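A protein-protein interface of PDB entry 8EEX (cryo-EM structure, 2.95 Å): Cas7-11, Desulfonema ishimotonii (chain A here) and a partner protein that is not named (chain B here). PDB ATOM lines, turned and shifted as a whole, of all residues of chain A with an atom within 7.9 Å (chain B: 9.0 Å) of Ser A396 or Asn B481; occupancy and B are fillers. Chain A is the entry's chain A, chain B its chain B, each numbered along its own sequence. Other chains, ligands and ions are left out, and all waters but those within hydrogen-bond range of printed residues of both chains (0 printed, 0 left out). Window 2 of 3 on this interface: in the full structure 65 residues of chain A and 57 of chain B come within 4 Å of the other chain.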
ATOM      1  N   GLU A  70      -8.110  10.078 -41.978  1.00  0.00           N
ATOM      2  CA  GLU A  70      -7.889  10.003 -40.537  1.00  0.00           C
ATOM      3  C   GLU A  70      -9.039  10.644 -39.772  1.00  0.00           C
ATOM      4  O   GLU A  70      -9.474  10.128 -38.736  1.00  0.00           O
ATOM      5  CB  GLU A  70      -6.576  10.690 -40.170  1.00  0.00           C
ATOM      6  CG  GLU A  70      -5.329   9.986 -40.662  1.00  0.00           C
ATOM      7  CD  GLU A  70      -4.064  10.720 -40.270  1.00  0.00           C
ATOM      8  OE1 GLU A  70      -3.946  11.120 -39.096  1.00  0.00           O
ATOM      9  OE2 GLU A  70      -3.184  10.895 -41.141  1.00  0.00           O
ATOM     10  N   THR A  74     -11.653   8.663 -37.080  1.00  0.00           N
ATOM     11  CA  THR A  74     -11.799   8.979 -35.664  1.00  0.00           C
ATOM     12  C   THR A  74     -13.252   9.280 -35.308  1.00  0.00           C
ATOM     13  O   THR A  74     -13.689   8.966 -34.196  1.00  0.00           O
ATOM     14  CB  THR A  74     -10.865  10.132 -35.273  1.00  0.00           C
ATOM     15  OG1 THR A  74     -10.861  10.294 -33.850  1.00  0.00           O
ATOM     16  CG2 THR A  74     -11.249  11.450 -35.921  1.00  0.00           C
ATOM     17  N   LEU A  75     -14.012   9.879 -36.227  1.00  0.00           N
ATOM     18  CA  LEU A  75     -15.435  10.096 -35.980  1.00  0.00           C
ATOM     19  C   LEU A  75     -16.196   8.778 -35.901  1.00  0.00           C
ATOM     20  O   LEU A  75     -17.057   8.604 -35.033  1.00  0.00           O
ATOM     21  CB  LEU A  75     -16.033  10.984 -37.070  1.00  0.00           C
ATOM     22  CG  LEU A  75     -15.496  12.409 -37.213  1.00  0.00           C
ATOM     23  CD1 LEU A  75     -16.162  13.103 -38.383  1.00  0.00           C
ATOM     24  CD2 LEU A  75     -15.701  13.213 -35.950  1.00  0.00           C
ATOM     25  N   SER A 105       0.809  15.788 -35.533  1.00  0.00           N
ATOM     26  CA  SER A 105       0.470  14.544 -34.860  1.00  0.00           C
ATOM     27  C   SER A 105      -0.529  13.743 -35.686  1.00  0.00           C
ATOM     28  O   SER A 105      -1.524  14.287 -36.171  1.00  0.00           O
ATOM     29  CB  SER A 105      -0.113  14.843 -33.483  1.00  0.00           C
ATOM     30  OG  SER A 105       0.899  15.235 -32.576  1.00  0.00           O
ATOM     31  N   THR A 106      -0.261  12.451 -35.851  1.00  0.00           N
ATOM     32  CA  THR A 106      -1.241  11.553 -36.442  1.00  0.00           C
ATOM     33  C   THR A 106      -2.338  11.232 -35.434  1.00  0.00           C
ATOM     34  O   THR A 106      -2.100  11.136 -34.230  1.00  0.00           O
ATOM     35  CB  THR A 106      -0.574  10.263 -36.940  1.00  0.00           C
ATOM     36  OG1 THR A 106      -1.559   9.403 -37.526  1.00  0.00           O
ATOM     37  CG2 THR A 106       0.148   9.511 -35.815  1.00  0.00           C
ATOM     38  N   LEU A 107      -3.558  11.089 -35.938  1.00  0.00           N
ATOM     39  CA  LEU A 107      -4.689  10.773 -35.082  1.00  0.00           C
ATOM     40  C   LEU A 107      -4.721   9.276 -34.791  1.00  0.00           C
ATOM     41  O   LEU A 107      -4.188   8.462 -35.550  1.00  0.00           O
ATOM     42  CB  LEU A 107      -5.992  11.210 -35.746  1.00  0.00           C
ATOM     43  CG  LEU A 107      -6.063  12.668 -36.222  1.00  0.00           C
ATOM     44  CD1 LEU A 107      -7.482  13.010 -36.610  1.00  0.00           C
ATOM     45  CD2 LEU A 107      -5.542  13.638 -35.178  1.00  0.00           C
ATOM     46  N   ARG A 108      -5.341   8.913 -33.667  1.00  0.00           N
ATOM     47  CA  ARG A 108      -5.571   7.513 -33.347  1.00  0.00           C
ATOM     48  C   ARG A 108      -7.021   7.278 -32.960  1.00  0.00           C
ATOM     49  O   ARG A 108      -7.682   8.137 -32.372  1.00  0.00           O
ATOM     50  CB  ARG A 108      -4.678   6.996 -32.209  1.00  0.00           C
ATOM     51  CG  ARG A 108      -5.157   7.332 -30.795  1.00  0.00           C
ATOM     52  CD  ARG A 108      -3.995   7.433 -29.825  1.00  0.00           C
ATOM     53  NE  ARG A 108      -3.702   6.120 -29.252  1.00  0.00           N
ATOM     54  CZ  ARG A 108      -2.551   5.463 -29.349  1.00  0.00           C
ATOM     55  NH1 ARG A 108      -1.540   5.916 -30.075  1.00  0.00           N
ATOM     56  NH2 ARG A 108      -2.420   4.297 -28.721  1.00  0.00           N
ATOM     57  N   TRP A 109      -7.488   6.083 -33.306  1.00  0.00           N
ATOM     58  CA  TRP A 109      -8.821   5.608 -32.979  1.00  0.00           C
ATOM     59  C   TRP A 109      -8.798   4.248 -32.294  1.00  0.00           C
ATOM     60  O   TRP A 109      -9.833   3.816 -31.774  1.00  0.00           O
ATOM     61  CB  TRP A 109      -9.676   5.549 -34.258  1.00  0.00           C
ATOM     62  CG  TRP A 109      -8.927   4.982 -35.428  1.00  0.00           C
ATOM     63  CD1 TRP A 109      -8.807   3.669 -35.777  1.00  0.00           C
ATOM     64  CD2 TRP A 109      -8.122   5.714 -36.358  1.00  0.00           C
ATOM     65  NE1 TRP A 109      -8.012   3.543 -36.885  1.00  0.00           N
ATOM     66  CE2 TRP A 109      -7.573   4.785 -37.259  1.00  0.00           C
ATOM     67  CE3 TRP A 109      -7.821   7.071 -36.521  1.00  0.00           C
ATOM     68  CZ2 TRP A 109      -6.749   5.162 -38.309  1.00  0.00           C
ATOM     69  CZ3 TRP A 109      -7.001   7.444 -37.567  1.00  0.00           C
ATOM     70  CH2 TRP A 109      -6.475   6.492 -38.447  1.00  0.00           C
ATOM     71  N   THR A 110      -7.658   3.559 -32.292  1.00  0.00           N
ATOM     72  CA  THR A 110      -7.461   2.298 -31.593  1.00  0.00           C
ATOM     73  C   THR A 110      -6.020   2.241 -31.108  1.00  0.00           C
ATOM     74  O   THR A 110      -5.165   2.995 -31.580  1.00  0.00           O
ATOM     75  CB  THR A 110      -7.740   1.067 -32.471  1.00  0.00           C
ATOM     76  OG1 THR A 110      -6.708   0.932 -33.457  1.00  0.00           O
ATOM     77  CG2 THR A 110      -9.126   1.096 -33.121  1.00  0.00           C
ATOM     78  N   ASP A 111      -5.766   1.353 -30.150  1.00  0.00           N
ATOM     79  CA  ASP A 111      -4.435   1.147 -29.590  1.00  0.00           C
ATOM     80  C   ASP A 111      -3.699  -0.048 -30.190  1.00  0.00           C
ATOM     81  O   ASP A 111      -2.546  -0.293 -29.821  1.00  0.00           O
ATOM     82  CB  ASP A 111      -4.537   0.973 -28.074  1.00  0.00           C
ATOM     83  CG  ASP A 111      -5.093   2.201 -27.387  1.00  0.00           C
ATOM     84  OD1 ASP A 111      -4.978   3.303 -27.961  1.00  0.00           O
ATOM     85  OD2 ASP A 111      -5.652   2.065 -26.279  1.00  0.00           O
ATOM     86  N   SER A 394       1.168  10.805 -31.372  1.00  0.00           N
ATOM     87  CA  SER A 394      -0.167  10.302 -31.677  1.00  0.00           C
ATOM     88  C   SER A 394      -1.158  10.870 -30.669  1.00  0.00           C
ATOM     89  O   SER A 394      -0.871  10.901 -29.469  1.00  0.00           O
ATOM     90  CB  SER A 394      -0.186   8.772 -31.653  1.00  0.00           C
ATOM     91  OG  SER A 394      -1.483   8.271 -31.907  1.00  0.00           O
ATOM     92  N   VAL A 395      -2.317  11.320 -31.156  1.00  0.00           N
ATOM     93  CA  VAL A 395      -3.299  12.036 -30.344  1.00  0.00           C
ATOM     94  C   VAL A 395      -4.691  11.528 -30.700  1.00  0.00           C
ATOM     95  O   VAL A 395      -4.945  11.145 -31.846  1.00  0.00           O
ATOM     96  CB  VAL A 395      -3.180  13.562 -30.551  1.00  0.00           C
ATOM     97  CG1 VAL A 395      -4.223  14.310 -29.736  1.00  0.00           C
ATOM     98  CG2 VAL A 395      -1.783  14.037 -30.186  1.00  0.00           C
ATOM     99  N   SER A 396      -5.592  11.516 -29.712  1.00  0.00           N
ATOM    100  CA  SER A 396      -6.897  10.871 -29.877  1.00  0.00           C
ATOM    101  C   SER A 396      -7.942  11.804 -30.486  1.00  0.00           C
ATOM    102  O   SER A 396      -8.620  11.433 -31.450  1.00  0.00           O
ATOM    103  CB  SER A 396      -7.386  10.349 -28.529  1.00  0.00           C
ATOM    104  OG  SER A 396      -7.543  11.409 -27.607  1.00  0.00           O
ATOM    105  N   ILE A 397      -8.107  13.002 -29.920  1.00  0.00           N
ATOM    106  CA  ILE A 397      -9.118  13.992 -30.315  1.00  0.00           C
ATOM    107  C   ILE A 397     -10.552  13.557 -30.007  1.00  0.00           C
ATOM    108  O   ILE A 397     -11.350  14.368 -29.524  1.00  0.00           O
ATOM    109  CB  ILE A 397      -8.962  14.345 -31.811  1.00  0.00           C
ATOM    110  CG1 ILE A 397      -7.519  14.811 -32.051  1.00  0.00           C
ATOM    111  CG2 ILE A 397     -10.031  15.383 -32.260  1.00  0.00           C
ATOM    112  CD1 ILE A 397      -7.280  15.652 -33.283  1.00  0.00           C
ATOM    113  N   GLY A 398     -10.905  12.301 -30.268  1.00  0.00           N
ATOM    114  CA  GLY A 398     -12.215  11.795 -29.915  1.00  0.00           C
ATOM    115  C   GLY A 398     -13.268  12.025 -30.985  1.00  0.00           C
ATOM    116  O   GLY A 398     -13.046  12.669 -32.011  1.00  0.00           O
ATOM    117  N   SER A 399     -14.452  11.467 -30.724  1.00  0.00           N
ATOM    118  CA  SER A 399     -15.517  11.420 -31.720  1.00  0.00           C
ATOM    119  C   SER A 399     -16.353  12.692 -31.784  1.00  0.00           C
ATOM    120  O   SER A 399     -17.048  12.900 -32.783  1.00  0.00           O
ATOM    121  CB  SER A 399     -16.435  10.232 -31.434  1.00  0.00           C
ATOM    122  OG  SER A 399     -17.427  10.102 -32.438  1.00  0.00           O
ATOM    123  N   ARG A 478      -4.528  27.023 -31.509  1.00  0.00           N
ATOM    124  CA  ARG A 478      -5.511  25.953 -31.643  1.00  0.00           C
ATOM    125  C   ARG A 478      -6.847  26.458 -32.171  1.00  0.00           C
ATOM    126  O   ARG A 478      -7.567  25.704 -32.835  1.00  0.00           O
ATOM    127  CB  ARG A 478      -5.674  25.239 -30.301  1.00  0.00           C
ATOM    128  CG  ARG A 478      -4.456  24.399 -29.948  1.00  0.00           C
ATOM    129  CD  ARG A 478      -4.659  23.509 -28.741  1.00  0.00           C
ATOM    130  NE  ARG A 478      -4.652  24.252 -27.481  1.00  0.00           N
ATOM    131  CZ  ARG A 478      -5.642  24.322 -26.598  1.00  0.00           C
ATOM    132  NH1 ARG A 478      -6.830  23.779 -26.825  1.00  0.00           N
ATOM    133  NH2 ARG A 478      -5.435  24.957 -25.450  1.00  0.00           N
ATOM    134  N   SER A 537     -14.353  20.693 -31.232  1.00  0.00           N
ATOM    135  CA  SER A 537     -15.037  19.744 -30.360  1.00  0.00           C
ATOM    136  C   SER A 537     -16.006  20.395 -29.382  1.00  0.00           C
ATOM    137  O   SER A 537     -16.921  19.715 -28.906  1.00  0.00           O
ATOM    138  CB  SER A 537     -14.011  18.921 -29.573  1.00  0.00           C
ATOM    139  OG  SER A 537     -13.498  19.651 -28.475  1.00  0.00           O
ATOM    140  N   GLU B 473       3.915  13.247 -26.119  1.00  0.00           N
ATOM    141  CA  GLU B 473       2.704  12.552 -26.530  1.00  0.00           C
ATOM    142  C   GLU B 473       1.619  12.665 -25.468  1.00  0.00           C
ATOM    143  O   GLU B 473       0.440  12.833 -25.796  1.00  0.00           O
ATOM    144  CB  GLU B 473       3.032  11.093 -26.828  1.00  0.00           C
ATOM    145  CG  GLU B 473       1.931  10.331 -27.529  1.00  0.00           C
ATOM    146  CD  GLU B 473       2.307   8.886 -27.777  1.00  0.00           C
ATOM    147  OE1 GLU B 473       3.037   8.621 -28.755  1.00  0.00           O
ATOM    148  OE2 GLU B 473       1.870   8.013 -27.000  1.00  0.00           O
ATOM    149  N   TRP B 474       1.990  12.562 -24.190  1.00  0.00           N
ATOM    150  CA  TRP B 474       1.031  12.840 -23.125  1.00  0.00           C
ATOM    151  C   TRP B 474       0.587  14.293 -23.161  1.00  0.00           C
ATOM    152  O   TRP B 474      -0.599  14.601 -22.991  1.00  0.00           O
ATOM    153  CB  TRP B 474       1.634  12.539 -21.758  1.00  0.00           C
ATOM    154  CG  TRP B 474       0.779  13.074 -20.648  1.00  0.00           C
ATOM    155  CD1 TRP B 474      -0.437  12.603 -20.253  1.00  0.00           C
ATOM    156  CD2 TRP B 474       1.049  14.217 -19.828  1.00  0.00           C
ATOM    157  NE1 TRP B 474      -0.928  13.360 -19.220  1.00  0.00           N
ATOM    158  CE2 TRP B 474      -0.037  14.360 -18.943  1.00  0.00           C
ATOM    159  CE3 TRP B 474       2.108  15.126 -19.748  1.00  0.00           C
ATOM    160  CZ2 TRP B 474      -0.096  15.371 -17.991  1.00  0.00           C
ATOM    161  CZ3 TRP B 474       2.048  16.129 -18.802  1.00  0.00           C
ATOM    162  CH2 TRP B 474       0.953  16.243 -17.936  1.00  0.00           C
ATOM    163  N   GLN B 475       1.542  15.206 -23.350  1.00  0.00           N
ATOM    164  CA  GLN B 475       1.272  16.629 -23.178  1.00  0.00           C
ATOM    165  C   GLN B 475       0.211  17.113 -24.157  1.00  0.00           C
ATOM    166  O   GLN B 475      -0.679  17.887 -23.786  1.00  0.00           O
ATOM    167  CB  GLN B 475       2.578  17.406 -23.339  1.00  0.00           C
ATOM    168  CG  GLN B 475       2.500  18.908 -23.127  1.00  0.00           C
ATOM    169  CD  GLN B 475       3.587  19.637 -23.887  1.00  0.00           C
ATOM    170  OE1 GLN B 475       4.624  19.984 -23.330  1.00  0.00           O
ATOM    171  NE2 GLN B 475       3.339  19.897 -25.163  1.00  0.00           N
ATOM    172  N   GLU B 476       0.291  16.681 -25.417  1.00  0.00           N
ATOM    173  CA  GLU B 476      -0.731  17.063 -26.388  1.00  0.00           C
ATOM    174  C   GLU B 476      -2.083  16.457 -26.035  1.00  0.00           C
ATOM    175  O   GLU B 476      -3.113  17.132 -26.122  1.00  0.00           O
ATOM    176  CB  GLU B 476      -0.304  16.642 -27.792  1.00  0.00           C
ATOM    177  CG  GLU B 476       0.824  17.483 -28.356  1.00  0.00           C
ATOM    178  CD  GLU B 476       1.123  17.182 -29.810  1.00  0.00           C
ATOM    179  OE1 GLU B 476       0.219  16.699 -30.522  1.00  0.00           O
ATOM    180  OE2 GLU B 476       2.262  17.450 -30.246  1.00  0.00           O
ATOM    181  N   ASN B 477      -2.102  15.183 -25.639  1.00  0.00           N
ATOM    182  CA  ASN B 477      -3.360  14.568 -25.230  1.00  0.00           C
ATOM    183  C   ASN B 477      -3.925  15.239 -23.988  1.00  0.00           C
ATOM    184  O   ASN B 477      -5.147  15.310 -23.821  1.00  0.00           O
ATOM    185  CB  ASN B 477      -3.157  13.073 -24.982  1.00  0.00           C
ATOM    186  CG  ASN B 477      -3.074  12.275 -26.268  1.00  0.00           C
ATOM    187  OD1 ASN B 477      -4.084  12.028 -26.923  1.00  0.00           O
ATOM    188  ND2 ASN B 477      -1.865  11.866 -26.633  1.00  0.00           N
ATOM    189  N   TYR B 478      -3.057  15.728 -23.101  1.00  0.00           N
ATOM    190  CA  TYR B 478      -3.522  16.479 -21.939  1.00  0.00           C
ATOM    191  C   TYR B 478      -4.128  17.817 -22.344  1.00  0.00           C
ATOM    192  O   TYR B 478      -5.189  18.204 -21.843  1.00  0.00           O
ATOM    193  CB  TYR B 478      -2.368  16.688 -20.960  1.00  0.00           C
ATOM    194  CG  TYR B 478      -2.656  17.713 -19.892  1.00  0.00           C
ATOM    195  CD1 TYR B 478      -3.517  17.435 -18.844  1.00  0.00           C
ATOM    196  CD2 TYR B 478      -2.045  18.954 -19.923  1.00  0.00           C
ATOM    197  CE1 TYR B 478      -3.773  18.371 -17.871  1.00  0.00           C
ATOM    198  CE2 TYR B 478      -2.293  19.892 -18.955  1.00  0.00           C
ATOM    199  CZ  TYR B 478      -3.158  19.596 -17.931  1.00  0.00           C
ATOM    200  OH  TYR B 478      -3.408  20.534 -16.960  1.00  0.00           O
ATOM    201  N   ILE B 479      -3.459  18.543 -23.240  1.00  0.00           N
ATOM    202  CA  ILE B 479      -3.919  19.878 -23.615  1.00  0.00           C
ATOM    203  C   ILE B 479      -5.276  19.802 -24.305  1.00  0.00           C
ATOM    204  O   ILE B 479      -6.112  20.702 -24.159  1.00  0.00           O
ATOM    205  CB  ILE B 479      -2.857  20.572 -24.490  1.00  0.00           C
ATOM    206  CG1 ILE B 479      -1.646  20.942 -23.624  1.00  0.00           C
ATOM    207  CG2 ILE B 479      -3.429  21.818 -25.165  1.00  0.00           C
ATOM    208  CD1 ILE B 479      -0.420  21.388 -24.391  1.00  0.00           C
ATOM    209  N   LEU B 480      -5.516  18.736 -25.072  1.00  0.00           N
ATOM    210  CA  LEU B 480      -6.786  18.593 -25.775  1.00  0.00           C
ATOM    211  C   LEU B 480      -7.884  17.965 -24.922  1.00  0.00           C
ATOM    212  O   LEU B 480      -9.064  18.214 -25.188  1.00  0.00           O
ATOM    213  CB  LEU B 480      -6.603  17.761 -27.046  1.00  0.00           C
ATOM    214  CG  LEU B 480      -6.131  18.534 -28.279  1.00  0.00           C
ATOM    215  CD1 LEU B 480      -4.665  18.835 -28.216  1.00  0.00           C
ATOM    216  CD2 LEU B 480      -6.453  17.762 -29.541  1.00  0.00           C
ATOM    217  N   ASN B 481      -7.537  17.154 -23.910  1.00  0.00           N
ATOM    218  CA  ASN B 481      -8.541  16.359 -23.209  1.00  0.00           C
ATOM    219  C   ASN B 481      -8.436  16.353 -21.690  1.00  0.00           C
ATOM    220  O   ASN B 481      -9.339  15.813 -21.042  1.00  0.00           O
ATOM    221  CB  ASN B 481      -8.487  14.899 -23.694  1.00  0.00           C
ATOM    222  CG  ASN B 481      -8.466  14.785 -25.198  1.00  0.00           C
ATOM    223  OD1 ASN B 481      -9.502  14.880 -25.854  1.00  0.00           O
ATOM    224  ND2 ASN B 481      -7.283  14.577 -25.756  1.00  0.00           N
ATOM    225  N   GLU B 482      -7.396  16.942 -21.099  1.00  0.00           N
ATOM    226  CA  GLU B 482      -7.192  16.880 -19.653  1.00  0.00           C
ATOM    227  C   GLU B 482      -7.229  15.433 -19.156  1.00  0.00           C
ATOM    228  O   GLU B 482      -6.315  14.657 -19.453  1.00  0.00           O
ATOM    229  CB  GLU B 482      -8.226  17.746 -18.920  1.00  0.00           C
ATOM    230  CG  GLU B 482      -8.033  19.247 -19.086  1.00  0.00           C
ATOM    231  CD  GLU B 482      -9.061  19.875 -20.004  1.00  0.00           C
ATOM    232  OE1 GLU B 482     -10.270  19.764 -19.708  1.00  0.00           O
ATOM    233  OE2 GLU B 482      -8.664  20.487 -21.016  1.00  0.00           O
ATOM    234  N   GLU B 483      -8.265  15.049 -18.397  1.00  0.00           N
ATOM    235  CA  GLU B 483      -8.278  13.730 -17.772  1.00  0.00           C
ATOM    236  C   GLU B 483      -8.372  12.596 -18.785  1.00  0.00           C
ATOM    237  O   GLU B 483      -8.119  11.441 -18.427  1.00  0.00           O
ATOM    238  CB  GLU B 483      -9.421  13.636 -16.759  1.00  0.00           C
ATOM    239  CG  GLU B 483     -10.837  13.604 -17.330  1.00  0.00           C
ATOM    240  CD  GLU B 483     -11.631  14.849 -16.992  1.00  0.00           C
ATOM    241  OE1 GLU B 483     -12.726  14.710 -16.406  1.00  0.00           O
ATOM    242  OE2 GLU B 483     -11.169  15.963 -17.315  1.00  0.00           O
ATOM    243  N   GLY B 484      -8.746  12.886 -20.033  1.00  0.00           N
ATOM    244  CA  GLY B 484      -8.697  11.868 -21.066  1.00  0.00           C
ATOM    245  C   GLY B 484      -7.295  11.371 -21.365  1.00  0.00           C
ATOM    246  O   GLY B 484      -7.142  10.324 -22.003  1.00  0.00           O
ATOM    247  N   SER B 485      -6.270  12.098 -20.922  1.00  0.00           N
ATOM    248  CA  SER B 485      -4.878  11.734 -21.159  1.00  0.00           C
ATOM    249  C   SER B 485      -4.333  10.734 -20.149  1.00  0.00           C
ATOM    250  O   SER B 485      -3.128  10.467 -20.170  1.00  0.00           O
ATOM    251  CB  SER B 485      -4.007  12.990 -21.138  1.00  0.00           C
ATOM    252  OG  SER B 485      -3.904  13.519 -19.824  1.00  0.00           O
ATOM    253  N   ALA B 486      -5.177  10.186 -19.269  1.00  0.00           N
ATOM    254  CA  ALA B 486      -4.675   9.415 -18.134  1.00  0.00           C
ATOM    255  C   ALA B 486      -3.861   8.204 -18.579  1.00  0.00           C
ATOM    256  O   ALA B 486      -2.844   7.871 -17.961  1.00  0.00           O
ATOM    257  CB  ALA B 486      -5.841   8.975 -17.252  1.00  0.00           C
ATOM    258  N   PHE B 488      -2.023   7.917 -21.253  1.00  0.00           N
ATOM    259  CA  PHE B 488      -0.706   8.379 -21.671  1.00  0.00           C
ATOM    260  C   PHE B 488       0.159   8.769 -20.482  1.00  0.00           C
ATOM    261  O   PHE B 488       1.382   8.598 -20.526  1.00  0.00           O
ATOM    262  CB  PHE B 488      -0.852   9.546 -22.645  1.00  0.00           C
ATOM    263  CG  PHE B 488      -1.523   9.172 -23.937  1.00  0.00           C
ATOM    264  CD1 PHE B 488      -0.788   8.634 -24.975  1.00  0.00           C
ATOM    265  CD2 PHE B 488      -2.881   9.354 -24.116  1.00  0.00           C
ATOM    266  CE1 PHE B 488      -1.389   8.285 -26.164  1.00  0.00           C
ATOM    267  CE2 PHE B 488      -3.489   9.006 -25.306  1.00  0.00           C
ATOM    268  CZ  PHE B 488      -2.741   8.471 -26.329  1.00  0.00           C
ATOM    269  N   THR B 694      -3.215  20.168 -13.816  1.00  0.00           N
ATOM    270  CA  THR B 694      -4.432  20.674 -13.190  1.00  0.00           C
ATOM    271  C   THR B 694      -5.059  19.623 -12.284  1.00  0.00           C
ATOM    272  O   THR B 694      -5.218  18.461 -12.666  1.00  0.00           O
ATOM    273  CB  THR B 694      -5.440  21.122 -14.246  1.00  0.00           C
ATOM    274  OG1 THR B 694      -5.566  20.118 -15.260  1.00  0.00           O
ATOM    275  CG2 THR B 694      -5.009  22.441 -14.871  1.00  0.00           C
ATOM    276  N   TYR B 738      -4.310   9.488 -12.238  1.00  0.00           N
ATOM    277  CA  TYR B 738      -4.192  10.844 -12.760  1.00  0.00           C
ATOM    278  C   TYR B 738      -4.496  11.901 -11.705  1.00  0.00           C
ATOM    279  O   TYR B 738      -3.975  13.018 -11.786  1.00  0.00           O
ATOM    280  CB  TYR B 738      -5.117  10.989 -13.973  1.00  0.00           C
ATOM    281  CG  TYR B 738      -5.225  12.373 -14.572  1.00  0.00           C
ATOM    282  CD1 TYR B 738      -6.151  13.286 -14.092  1.00  0.00           C
ATOM    283  CD2 TYR B 738      -4.407  12.766 -15.618  1.00  0.00           C
ATOM    284  CE1 TYR B 738      -6.259  14.540 -14.634  1.00  0.00           C
ATOM    285  CE2 TYR B 738      -4.508  14.023 -16.165  1.00  0.00           C
ATOM    286  CZ  TYR B 738      -5.434  14.906 -15.668  1.00  0.00           C
ATOM    287  OH  TYR B 738      -5.541  16.163 -16.211  1.00  0.00           O
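OG of Ser A105 sits at hydrogen-bond distance from OE1 of Glu B476 (2.6 Å).
The backbone carbonyl oxygen (O) of Ser A394 sits at hydrogen-bond distance from the side-chain amide nitrogen (ND2) of Asn B477, at 3.2 Å.
The backbone NH (N) of Ser A396 is in hydrogen-bond range of the side-chain amide oxygen (OD1) of Asn B477 (3.2 Å).
Of the 18 printed residues of chain A, 6 touch a printed residue of chain B.
Printed residues of chain A that touch a printed residue of chain B: Ser A105, Arg A108, Ser A394, Val A395, Ser A396 and Arg A478.
Along chain A the printed residues that touch a printed residue of chain B span positions 105 to 478.
Among the printed residues, 9 pairs touch across the chains.
Among the printed residues, no Asp or Glu carboxylate lies within 4 Å of a Lys or Arg side-chain nitrogen of the other chain.
CD of Arg A108 touches CZ of Phe B488, at 3.9 Å.
Ser A394 touches Glu B473.
CG2 of Val A395 touches OE1 of Glu B476, 3.3 Å away.
OD1 of Asn B477 touches CA of Val A395, 3.5 Å away.
Ser A396 touches Asn B481.
NE of Arg A478 touches CG2 of Ile B479, 3.6 Å away.
O of Ser A396 sits at hydrogen-bond distance from OG1 of Thr A74, 3.5 Å away.
N of Val A395 is in hydrogen-bond range of O of Thr A106 (3.1 Å).
The side-chain carboxylate (OD1) of Asp A111 is in salt-bridge range of the guanidinium group (NH2) of Arg A108 (2.8 Å).
The side-chain hydroxyl of Ser A394 sits at hydrogen-bond distance from the guanidinium group of Arg A108 (3.0 Å).
The backbone carbonyl oxygen of Val A395 sits at hydrogen-bond distance from the backbone NH of Arg A108 (2.9 Å).
The side-chain amide nitrogen (ND2) of Asn B477 sits at hydrogen-bond distance from the backbone carbonyl oxygen (O) of Glu B473 (2.6 Å).
Printed residues of chain B within 4 Å of Arg A108: Phe B488 (3.9 Å).
Of chain B, only Glu B476 (3.3 Å) and Asn B477 (3.5 Å) come within 4 Å of Val A395.
Of chain B, only Asn B477 and Asn B481 come within 4 Å of Ser A396.
No residue of chain B comes within 4 Å of Gly A398.
Of the printed residues of chain A, Asn B477 touches Ser A394, Val A395 and Ser A396.
Of chain A, only Ser A396 (3.7 Å) comes within 4 Å of Asn B481.
Of the printed residues of chain A, Phe B488 touches Arg A108.
Thr B694 touches none of the printed residues of chain A.
The nearest printed residue of chain A that does not touch Phe B488 is Ser A394 (4.2 Å).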
